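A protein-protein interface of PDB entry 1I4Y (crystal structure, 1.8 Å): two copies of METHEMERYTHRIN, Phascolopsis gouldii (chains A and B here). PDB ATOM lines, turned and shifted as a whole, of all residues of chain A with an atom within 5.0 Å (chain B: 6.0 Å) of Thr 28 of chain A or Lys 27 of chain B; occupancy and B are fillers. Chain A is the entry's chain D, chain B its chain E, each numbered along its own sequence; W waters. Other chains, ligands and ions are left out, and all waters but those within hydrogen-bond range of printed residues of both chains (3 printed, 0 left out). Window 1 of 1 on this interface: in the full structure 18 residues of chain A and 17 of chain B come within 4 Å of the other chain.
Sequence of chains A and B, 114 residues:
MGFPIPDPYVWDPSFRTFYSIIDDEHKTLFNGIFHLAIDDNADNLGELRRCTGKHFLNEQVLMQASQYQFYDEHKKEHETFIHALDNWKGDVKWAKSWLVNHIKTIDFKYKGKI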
ATOM      1  N   ASP A  24      28.452   7.549 -18.980  1.00  0.00           N
ATOM      2  CA  ASP A  24      28.134   6.407 -19.827  1.00  0.00           C
ATOM      3  C   ASP A  24      29.158   5.293 -19.662  1.00  0.00           C
ATOM      4  O   ASP A  24      28.828   4.111 -19.785  1.00  0.00           O
ATOM      5  CB  ASP A  24      28.033   6.840 -21.293  1.00  0.00           C
ATOM      6  CG  ASP A  24      26.792   7.665 -21.564  1.00  0.00           C
ATOM      7  OD1 ASP A  24      26.648   8.187 -22.680  1.00  0.00           O
ATOM      8  OD2 ASP A  24      25.957   7.799 -20.646  1.00  0.00           O
ATOM      9  N   GLU A  25      30.405   5.667 -19.384  1.00  0.00           N
ATOM     10  CA  GLU A  25      31.445   4.667 -19.172  1.00  0.00           C
ATOM     11  C   GLU A  25      31.213   4.025 -17.798  1.00  0.00           C
ATOM     12  O   GLU A  25      31.359   2.815 -17.637  1.00  0.00           O
ATOM     13  CB  GLU A  25      32.844   5.290 -19.299  1.00  0.00           C
ATOM     14  CG  GLU A  25      33.175   5.724 -20.730  1.00  0.00           C
ATOM     15  CD  GLU A  25      34.550   6.377 -20.876  1.00  0.00           C
ATOM     16  OE1 GLU A  25      34.973   6.608 -22.024  1.00  0.00           O
ATOM     17  OE2 GLU A  25      35.202   6.672 -19.859  1.00  0.00           O
ATOM     18  N   HIS A  26      30.817   4.833 -16.819  1.00  0.00           N
ATOM     19  CA  HIS A  26      30.526   4.321 -15.484  1.00  0.00           C
ATOM     20  C   HIS A  26      29.396   3.283 -15.518  1.00  0.00           C
ATOM     21  O   HIS A  26      29.395   2.336 -14.727  1.00  0.00           O
ATOM     22  CB  HIS A  26      30.121   5.453 -14.554  1.00  0.00           C
ATOM     23  CG  HIS A  26      31.260   6.302 -14.102  1.00  0.00           C
ATOM     24  ND1 HIS A  26      31.076   7.463 -13.386  1.00  0.00           N
ATOM     25  CD2 HIS A  26      32.599   6.145 -14.221  1.00  0.00           C
ATOM     26  CE1 HIS A  26      32.248   7.983 -13.081  1.00  0.00           C
ATOM     27  NE2 HIS A  26      33.195   7.203 -13.578  1.00  0.00           N
ATOM     28  N   LYS A  27      28.433   3.473 -16.418  1.00  0.00           N
ATOM     29  CA  LYS A  27      27.324   2.538 -16.566  1.00  0.00           C
ATOM     30  C   LYS A  27      27.836   1.155 -16.970  1.00  0.00           C
ATOM     31  O   LYS A  27      27.254   0.140 -16.592  1.00  0.00           O
ATOM     32  CB  LYS A  27      26.323   3.044 -17.610  1.00  0.00           C
ATOM     33  CG  LYS A  27      25.653   4.358 -17.203  1.00  0.00           C
ATOM     34  CD  LYS A  27      24.834   4.949 -18.321  1.00  0.00           C
ATOM     35  CE  LYS A  27      24.285   6.313 -17.921  1.00  0.00           C
ATOM     36  NZ  LYS A  27      23.701   7.013 -19.102  1.00  0.00           N
ATOM     37  N   THR A  28      28.925   1.129 -17.739  1.00  0.00           N
ATOM     38  CA  THR A  28      29.511  -0.130 -18.182  1.00  0.00           C
ATOM     39  C   THR A  28      30.255  -0.831 -17.054  1.00  0.00           C
ATOM     40  O   THR A  28      30.351  -2.053 -17.046  1.00  0.00           O
ATOM     41  CB  THR A  28      30.457   0.060 -19.406  1.00  0.00           C
ATOM     42  OG1 THR A  28      31.635   0.767 -19.008  1.00  0.00           O
ATOM     43  CG2 THR A  28      29.756   0.864 -20.500  1.00  0.00           C
ATOM     44  N   LEU A  29      30.771  -0.068 -16.093  1.00  0.00           N
ATOM     45  CA  LEU A  29      31.495  -0.685 -14.986  1.00  0.00           C
ATOM     46  C   LEU A  29      30.511  -1.400 -14.075  1.00  0.00           C
ATOM     47  O   LEU A  29      30.746  -2.538 -13.664  1.00  0.00           O
ATOM     48  CB  LEU A  29      32.359   0.335 -14.221  1.00  0.00           C
ATOM     49  CG  LEU A  29      33.424   1.037 -15.090  1.00  0.00           C
ATOM     50  CD1 LEU A  29      34.503   1.702 -14.243  1.00  0.00           C
ATOM     51  CD2 LEU A  29      34.053   0.018 -16.030  1.00  0.00           C
ATOM     52  N   PHE A  30      29.373  -0.756 -13.819  1.00  0.00           N
ATOM     53  CA  PHE A  30      28.341  -1.372 -12.986  1.00  0.00           C
ATOM     54  C   PHE A  30      27.852  -2.664 -13.611  1.00  0.00           C
ATOM     55  O   PHE A  30      27.752  -3.688 -12.926  1.00  0.00           O
ATOM     56  CB  PHE A  30      27.162  -0.427 -12.782  1.00  0.00           C
ATOM     57  CG  PHE A  30      27.383   0.585 -11.702  1.00  0.00           C
ATOM     58  CD1 PHE A  30      27.973   1.816 -11.994  1.00  0.00           C
ATOM     59  CD2 PHE A  30      26.975   0.324 -10.392  1.00  0.00           C
ATOM     60  CE1 PHE A  30      28.151   2.781 -10.999  1.00  0.00           C
ATOM     61  CE2 PHE A  30      27.152   1.280  -9.384  1.00  0.00           C
ATOM     62  CZ  PHE A  30      27.743   2.516  -9.695  1.00  0.00           C
ATOM     63  N   ASN A  31      27.568  -2.616 -14.917  1.00  0.00           N
ATOM     64  CA  ASN A  31      27.088  -3.789 -15.660  1.00  0.00           C
ATOM     65  C   ASN A  31      28.111  -4.912 -15.603  1.00  0.00           C
ATOM     66  O   ASN A  31      27.739  -6.092 -15.560  1.00  0.00           O
ATOM     67  CB  ASN A  31      26.815  -3.442 -17.128  1.00  0.00           C
ATOM     68  CG  ASN A  31      26.227  -4.613 -17.903  1.00  0.00           C
ATOM     69  OD1 ASN A  31      25.109  -5.033 -17.645  1.00  0.00           O
ATOM     70  ND2 ASN A  31      26.985  -5.154 -18.840  1.00  0.00           N
ATOM     71  N   GLY A  32      29.394  -4.535 -15.631  1.00  0.00           N
ATOM     72  CA  GLY A  32      30.474  -5.509 -15.587  1.00  0.00           C
ATOM     73  C   GLY A  32      30.516  -6.254 -14.268  1.00  0.00           C
ATOM     74  O   GLY A  32      30.619  -7.489 -14.221  1.00  0.00           O
ATOM     75  N   GLU A  47      35.408  -8.605 -19.675  1.00  0.00           N
ATOM     76  CA  GLU A  47      34.502  -7.546 -20.124  1.00  0.00           C
ATOM     77  C   GLU A  47      34.676  -6.358 -19.183  1.00  0.00           C
ATOM     78  O   GLU A  47      34.845  -5.228 -19.639  1.00  0.00           O
ATOM     79  CB  GLU A  47      33.049  -8.029 -20.098  1.00  0.00           C
ATOM     80  CG  GLU A  47      32.040  -7.070 -20.748  1.00  0.00           C
ATOM     81  CD  GLU A  47      32.171  -6.971 -22.272  1.00  0.00           C
ATOM     82  OE1 GLU A  47      31.741  -5.941 -22.837  1.00  0.00           O
ATOM     83  OE2 GLU A  47      32.661  -7.927 -22.915  1.00  0.00           O
ATOM     84  N   ARG A  50      38.230  -4.765 -19.588  1.00  0.00           N
ATOM     85  CA  ARG A  50      38.340  -3.922 -20.777  1.00  0.00           C
ATOM     86  C   ARG A  50      37.673  -2.560 -20.536  1.00  0.00           C
ATOM     87  O   ARG A  50      38.276  -1.521 -20.796  1.00  0.00           O
ATOM     88  CB  ARG A  50      37.691  -4.582 -22.000  1.00  0.00           C
ATOM     89  CG  ARG A  50      37.619  -3.636 -23.216  1.00  0.00           C
ATOM     90  CD  ARG A  50      36.911  -4.253 -24.422  1.00  0.00           C
ATOM     91  NE  ARG A  50      35.474  -4.453 -24.223  1.00  0.00           N
ATOM     92  CZ  ARG A  50      34.578  -3.475 -24.102  1.00  0.00           C
ATOM     93  NH1 ARG A  50      33.294  -3.763 -23.939  1.00  0.00           N
ATOM     94  NH2 ARG A  50      34.951  -2.210 -24.134  1.00  0.00           N
ATOM     95  N   CYS A  51      36.433  -2.580 -20.042  1.00  0.00           N
ATOM     96  CA  CYS A  51      35.689  -1.340 -19.789  1.00  0.00           C
ATOM     97  C   CYS A  51      36.330  -0.512 -18.688  1.00  0.00           C
ATOM     98  O   CYS A  51      36.218   0.716 -18.682  1.00  0.00           O
ATOM     99  CB  CYS A  51      34.227  -1.634 -19.433  1.00  0.00           C
ATOM    100  SG  CYS A  51      33.300  -2.405 -20.747  1.00  0.00           S
ATOM    101  N   TRP B  11      21.978  -5.031 -19.770  1.00  0.00           N
ATOM    102  CA  TRP B  11      22.644  -5.679 -20.905  1.00  0.00           C
ATOM    103  C   TRP B  11      23.354  -6.940 -20.425  1.00  0.00           C
ATOM    104  O   TRP B  11      23.807  -6.994 -19.283  1.00  0.00           O
ATOM    105  CB  TRP B  11      23.682  -4.710 -21.485  1.00  0.00           C
ATOM    106  CG  TRP B  11      24.502  -5.220 -22.654  1.00  0.00           C
ATOM    107  CD1 TRP B  11      24.308  -4.926 -23.973  1.00  0.00           C
ATOM    108  CD2 TRP B  11      25.705  -6.010 -22.594  1.00  0.00           C
ATOM    109  NE1 TRP B  11      25.323  -5.466 -24.736  1.00  0.00           N
ATOM    110  CE2 TRP B  11      26.191  -6.134 -23.915  1.00  0.00           C
ATOM    111  CE3 TRP B  11      26.427  -6.611 -21.545  1.00  0.00           C
ATOM    112  CZ2 TRP B  11      27.360  -6.840 -24.220  1.00  0.00           C
ATOM    113  CZ3 TRP B  11      27.607  -7.319 -21.864  1.00  0.00           C
ATOM    114  CH2 TRP B  11      28.050  -7.418 -23.188  1.00  0.00           C
ATOM    115  N   ILE B  22      30.123  -0.059 -29.573  1.00  0.00           N
ATOM    116  CA  ILE B  22      28.703  -0.360 -29.738  1.00  0.00           C
ATOM    117  C   ILE B  22      28.116  -1.051 -28.518  1.00  0.00           C
ATOM    118  O   ILE B  22      27.107  -0.606 -27.977  1.00  0.00           O
ATOM    119  CB  ILE B  22      28.469  -1.280 -30.962  1.00  0.00           C
ATOM    120  CG1 ILE B  22      28.954  -0.599 -32.244  1.00  0.00           C
ATOM    121  CG2 ILE B  22      26.999  -1.654 -31.075  1.00  0.00           C
ATOM    122  CD1 ILE B  22      28.306   0.739 -32.527  1.00  0.00           C
ATOM    123  N   ASP B  23      28.762  -2.135 -28.087  1.00  0.00           N
ATOM    124  CA  ASP B  23      28.314  -2.901 -26.937  1.00  0.00           C
ATOM    125  C   ASP B  23      28.301  -2.040 -25.688  1.00  0.00           C
ATOM    126  O   ASP B  23      27.413  -2.166 -24.849  1.00  0.00           O
ATOM    127  CB  ASP B  23      29.191  -4.148 -26.730  1.00  0.00           C
ATOM    128  CG  ASP B  23      29.039  -5.175 -27.862  1.00  0.00           C
ATOM    129  OD1 ASP B  23      28.045  -5.109 -28.619  1.00  0.00           O
ATOM    130  OD2 ASP B  23      29.922  -6.050 -28.010  1.00  0.00           O
ATOM    131  N   ASP B  24      29.288  -1.162 -25.552  1.00  0.00           N
ATOM    132  CA  ASP B  24      29.324  -0.289 -24.385  1.00  0.00           C
ATOM    133  C   ASP B  24      28.160   0.711 -24.468  1.00  0.00           C
ATOM    134  O   ASP B  24      27.487   0.965 -23.468  1.00  0.00           O
ATOM    135  CB  ASP B  24      30.695   0.389 -24.229  1.00  0.00           C
ATOM    136  CG  ASP B  24      31.775  -0.583 -23.747  1.00  0.00           C
ATOM    137  OD1 ASP B  24      32.965  -0.203 -23.744  1.00  0.00           O
ATOM    138  OD2 ASP B  24      31.439  -1.730 -23.359  1.00  0.00           O
ATOM    139  N   GLU B  25      27.864   1.201 -25.669  1.00  0.00           N
ATOM    140  CA  GLU B  25      26.743   2.120 -25.847  1.00  0.00           C
ATOM    141  C   GLU B  25      25.414   1.409 -25.551  1.00  0.00           C
ATOM    142  O   GLU B  25      24.544   1.966 -24.882  1.00  0.00           O
ATOM    143  CB  GLU B  25      26.760   2.715 -27.250  1.00  0.00           C
ATOM    144  CG  GLU B  25      27.908   3.711 -27.416  1.00  0.00           C
ATOM    145  CD  GLU B  25      28.060   4.271 -28.814  1.00  0.00           C
ATOM    146  OE1 GLU B  25      28.877   5.203 -28.952  1.00  0.00           O
ATOM    147  OE2 GLU B  25      27.394   3.794 -29.767  1.00  0.00           O
ATOM    148  N   HIS B  26      25.282   0.168 -26.015  1.00  0.00           N
ATOM    149  CA  HIS B  26      24.077  -0.622 -25.764  1.00  0.00           C
ATOM    150  C   HIS B  26      23.819  -0.775 -24.271  1.00  0.00           C
ATOM    151  O   HIS B  26      22.676  -0.747 -23.837  1.00  0.00           O
ATOM    152  CB  HIS B  26      24.211  -2.003 -26.395  1.00  0.00           C
ATOM    153  CG  HIS B  26      24.002  -2.011 -27.869  1.00  0.00           C
ATOM    154  ND1 HIS B  26      24.300  -3.101 -28.654  1.00  0.00           N
ATOM    155  CD2 HIS B  26      23.499  -1.075 -28.704  1.00  0.00           C
ATOM    156  CE1 HIS B  26      23.993  -2.837 -29.910  1.00  0.00           C
ATOM    157  NE2 HIS B  26      23.504  -1.612 -29.969  1.00  0.00           N
ATOM    158  N   LYS B  27      24.884  -0.914 -23.483  1.00  0.00           N
ATOM    159  CA  LYS B  27      24.749  -1.050 -22.037  1.00  0.00           C
ATOM    160  C   LYS B  27      24.068   0.172 -21.432  1.00  0.00           C
ATOM    161  O   LYS B  27      23.325   0.046 -20.454  1.00  0.00           O
ATOM    162  CB  LYS B  27      26.122  -1.275 -21.380  1.00  0.00           C
ATOM    163  CG  LYS B  27      26.787  -2.608 -21.758  1.00  0.00           C
ATOM    164  CD  LYS B  27      28.198  -2.718 -21.222  1.00  0.00           C
ATOM    165  CE  LYS B  27      28.947  -3.886 -21.872  1.00  0.00           C
ATOM    166  NZ  LYS B  27      30.400  -3.893 -21.522  1.00  0.00           N
ATOM    167  N   THR B  28      24.314   1.351 -22.010  1.00  0.00           N
ATOM    168  CA  THR B  28      23.712   2.589 -21.500  1.00  0.00           C
ATOM    169  C   THR B  28      22.223   2.646 -21.826  1.00  0.00           C
ATOM    170  O   THR B  28      21.444   3.207 -21.055  1.00  0.00           O
ATOM    171  CB  THR B  28      24.428   3.856 -22.063  1.00  0.00           C
ATOM    172  OG1 THR B  28      24.114   4.016 -23.452  1.00  0.00           O
ATOM    173  CG2 THR B  28      25.948   3.720 -21.915  1.00  0.00           C
ATOM    174  N   LEU B  29      21.833   2.062 -22.963  1.00  0.00           N
ATOM    175  CA  LEU B  29      20.427   2.031 -23.372  1.00  0.00           C
ATOM    176  C   LEU B  29      19.592   1.177 -22.412  1.00  0.00           C
ATOM    177  O   LEU B  29      18.497   1.576 -22.010  1.00  0.00           O
ATOM    178  CB  LEU B  29      20.268   1.522 -24.803  1.00  0.00           C
ATOM    179  CG  LEU B  29      21.005   2.276 -25.909  1.00  0.00           C
ATOM    180  CD1 LEU B  29      20.304   2.035 -27.230  1.00  0.00           C
ATOM    181  CD2 LEU B  29      21.048   3.757 -25.632  1.00  0.00           C
ATOM    182  N   PHE B  30      20.118   0.016 -22.030  1.00  0.00           N
ATOM    183  CA  PHE B  30      19.418  -0.861 -21.106  1.00  0.00           C
ATOM    184  C   PHE B  30      19.222  -0.174 -19.766  1.00  0.00           C
ATOM    185  O   PHE B  30      18.127  -0.208 -19.196  1.00  0.00           O
ATOM    186  CB  PHE B  30      20.193  -2.175 -20.897  1.00  0.00           C
ATOM    187  CG  PHE B  30      19.963  -3.199 -21.966  1.00  0.00           C
ATOM    188  CD1 PHE B  30      20.716  -3.193 -23.124  1.00  0.00           C
ATOM    189  CD2 PHE B  30      18.991  -4.188 -21.806  1.00  0.00           C
ATOM    190  CE1 PHE B  30      20.517  -4.160 -24.114  1.00  0.00           C
ATOM    191  CE2 PHE B  30      18.789  -5.159 -22.796  1.00  0.00           C
ATOM    192  CZ  PHE B  30      19.553  -5.138 -23.946  1.00  0.00           C
ATOM    193  N   ASN B  31      20.283   0.460 -19.271  1.00  0.00           N
ATOM    194  CA  ASN B  31      20.225   1.159 -17.990  1.00  0.00           C
ATOM    195  C   ASN B  31      19.240   2.338 -18.043  1.00  0.00           C
ATOM    196  O   ASN B  31      18.570   2.650 -17.048  1.00  0.00           O
ATOM    197  CB  ASN B  31      21.617   1.642 -17.578  1.00  0.00           C
ATOM    198  CG  ASN B  31      21.635   2.224 -16.200  1.00  0.00           C
ATOM    199  OD1 ASN B  31      21.459   1.516 -15.224  1.00  0.00           O
ATOM    200  ND2 ASN B  31      21.814   3.521 -16.108  1.00  0.00           N
ATOM    201  N   GLY B  32      19.158   2.988 -19.205  1.00  0.00           N
ATOM    202  CA  GLY B  32      18.240   4.104 -19.393  1.00  0.00           C
ATOM    203  C   GLY B  32      16.794   3.658 -19.272  1.00  0.00           C
ATOM    204  O   GLY B  32      15.997   4.285 -18.564  1.00  0.00           O
HETATM  205  O   HOH W   1      30.796  -4.014 -18.817  1.00  0.00           O
HETATM  206  O   HOH W   2      31.348  -7.398 -25.191  1.00  0.00           O
HETATM  207  O   HOH W   3      21.422   5.644 -19.833  1.00  0.00           O
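Among the printed residues, merely in contact across the chains: Asp 24 of chain A with Thr 28 of chain B (3.6 Å), Asn 31 of chain A with Lys 27 of chain B (3.6 Å), Thr 28 of chain A with Asp 24 of chain B (3.7 Å), Arg 50 of chain A with Lys 27 of chain B (3.8 Å), Lys 27 of chain A with Thr 28 of chain B (3.9 Å), Thr 28 of chain A with Lys 27 of chain B (3.97 Å) and Glu 47 of chain A with Trp 11 of chain B (3.99 Å).
Of chain B, only Asp 24 and Lys 27 come within 4 Å of Thr 28 of chain A. Of chain A, only Thr 28 (3.97 Å), Asn 31 (3.6 Å), Glu 47 (2.8 Å), Arg 50 (3.8 Å) and Cys 51 (3.4 Å) come within 4 Å of Lys 27 of chain B. Printed residues of chain B within 4 Å of Glu 47 of chain A: Trp 11 and Lys 27. Printed residues of chain A within 4 Å of Thr 28 of chain B: Asp 24 and Lys 27. Gly 32 of chain A touches none of the printed residues of chain B. Glu 25 of chain A touches none of the printed residues of chain B. The nearest residue of chain B that does not touch Thr 28 of chain A is Thr 28 of chain B (5.0 Å). The nearest printed residue of chain A that does not touch Lys 27 of chain B is Lys 27 of chain A (5.1 Å).
Hydrophobic or aromatic side chains of chain B that line the printed part of chain A: Trp 11. Along chain B the printed residues that touch a printed residue of chain A span positions 11 to 28. Of the 12 printed residues of chain A, 7 touch a printed residue of chain B. Along chain A the printed residues that touch a printed residue of chain B span positions 24 to 51.
OD2 of Asp 24 of chain B lies within salt-bridge range of NH1 of Arg 50 of chain A, 2.8 Å away. The side-chain sulfur (SG) of Cys 51 of chain A sits at hydrogen-bond distance from the side-chain amino group (NZ) of Lys 27 of chain B, 3.4 Å away. The side-chain carboxylate (OD2) of Asp 24 of chain B sits at hydrogen-bond distance from the side-chain sulfur (SG) of Cys 51 of chain A, 3.3 Å away. OD1 of Asn 31 of chain A sits close to O of Trp 11 of chain B (2.9 Å). The side-chain carboxylate (OE1) of Glu 47 of chain A lies within salt-bridge range of the side-chain amino group (NZ) of Lys 27 of chain B (2.8 Å).
Water W1 lies within hydrogen-bond range of O of Thr 28 of chain A (2.7 Å), NZ of Lys 27 of chain B (2.7 Å) and SG of Cys 51 of chain A (3.5 Å). Water W2 lies within hydrogen-bond range of OE2 of Glu 47 of chain A (2.7 Å) and OD2 of Asp 23 of chain B (3.4 Å). Water W3 lies within hydrogen-bond range of O of Thr 28 of chain B (2.7 Å) and NZ of Lys 27 of chain A (2.8 Å).
Asp 24 of chain A touches Thr 28 of chain B, and with the chains exchanged Thr 28 of chain A touches Asp 24 of chain B. Lys 27 of chain A touches Thr 28 of chain B, and with the chains exchanged Thr 28 of chain A touches Lys 27 of chain B. Asn 31 of chain A touches Lys 27 of chain B, but with the chains exchanged Lys 27 of chain A does not touch Asn 31 of chain B (4.01 Å). Positions printed for both chains: 24, 25, 26, 27, 28, 29, 30, 31 and 32. Of the 12 pairs that touch across the chains among the printed residues, 4 have their exchanged pair printed and touching as well.
NH1 of Arg 50 of chain A sits at hydrogen-bond distance from SG of Cys 51 of chain A (3.5 Å). The side-chain carboxylate (OD2) of Asp 24 of chain A lies within salt-bridge range of the side-chain amino group (NZ) of Lys 27 of chain A (2.8 Å). SG of Cys 51 of chain A sits at hydrogen-bond distance from O of Glu 47 of chain A (3.4 Å). OE1 of Glu 47 of chain A is in salt-bridge range of NH1 of Arg 50 of chain A (2.9 Å). O of Glu 25 of chain A sits at hydrogen-bond distance from OG1 of Thr 28 of chain A (2.5 Å). OG1 of Thr 28 of chain B sits at hydrogen-bond distance from O of Glu 25 of chain B.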
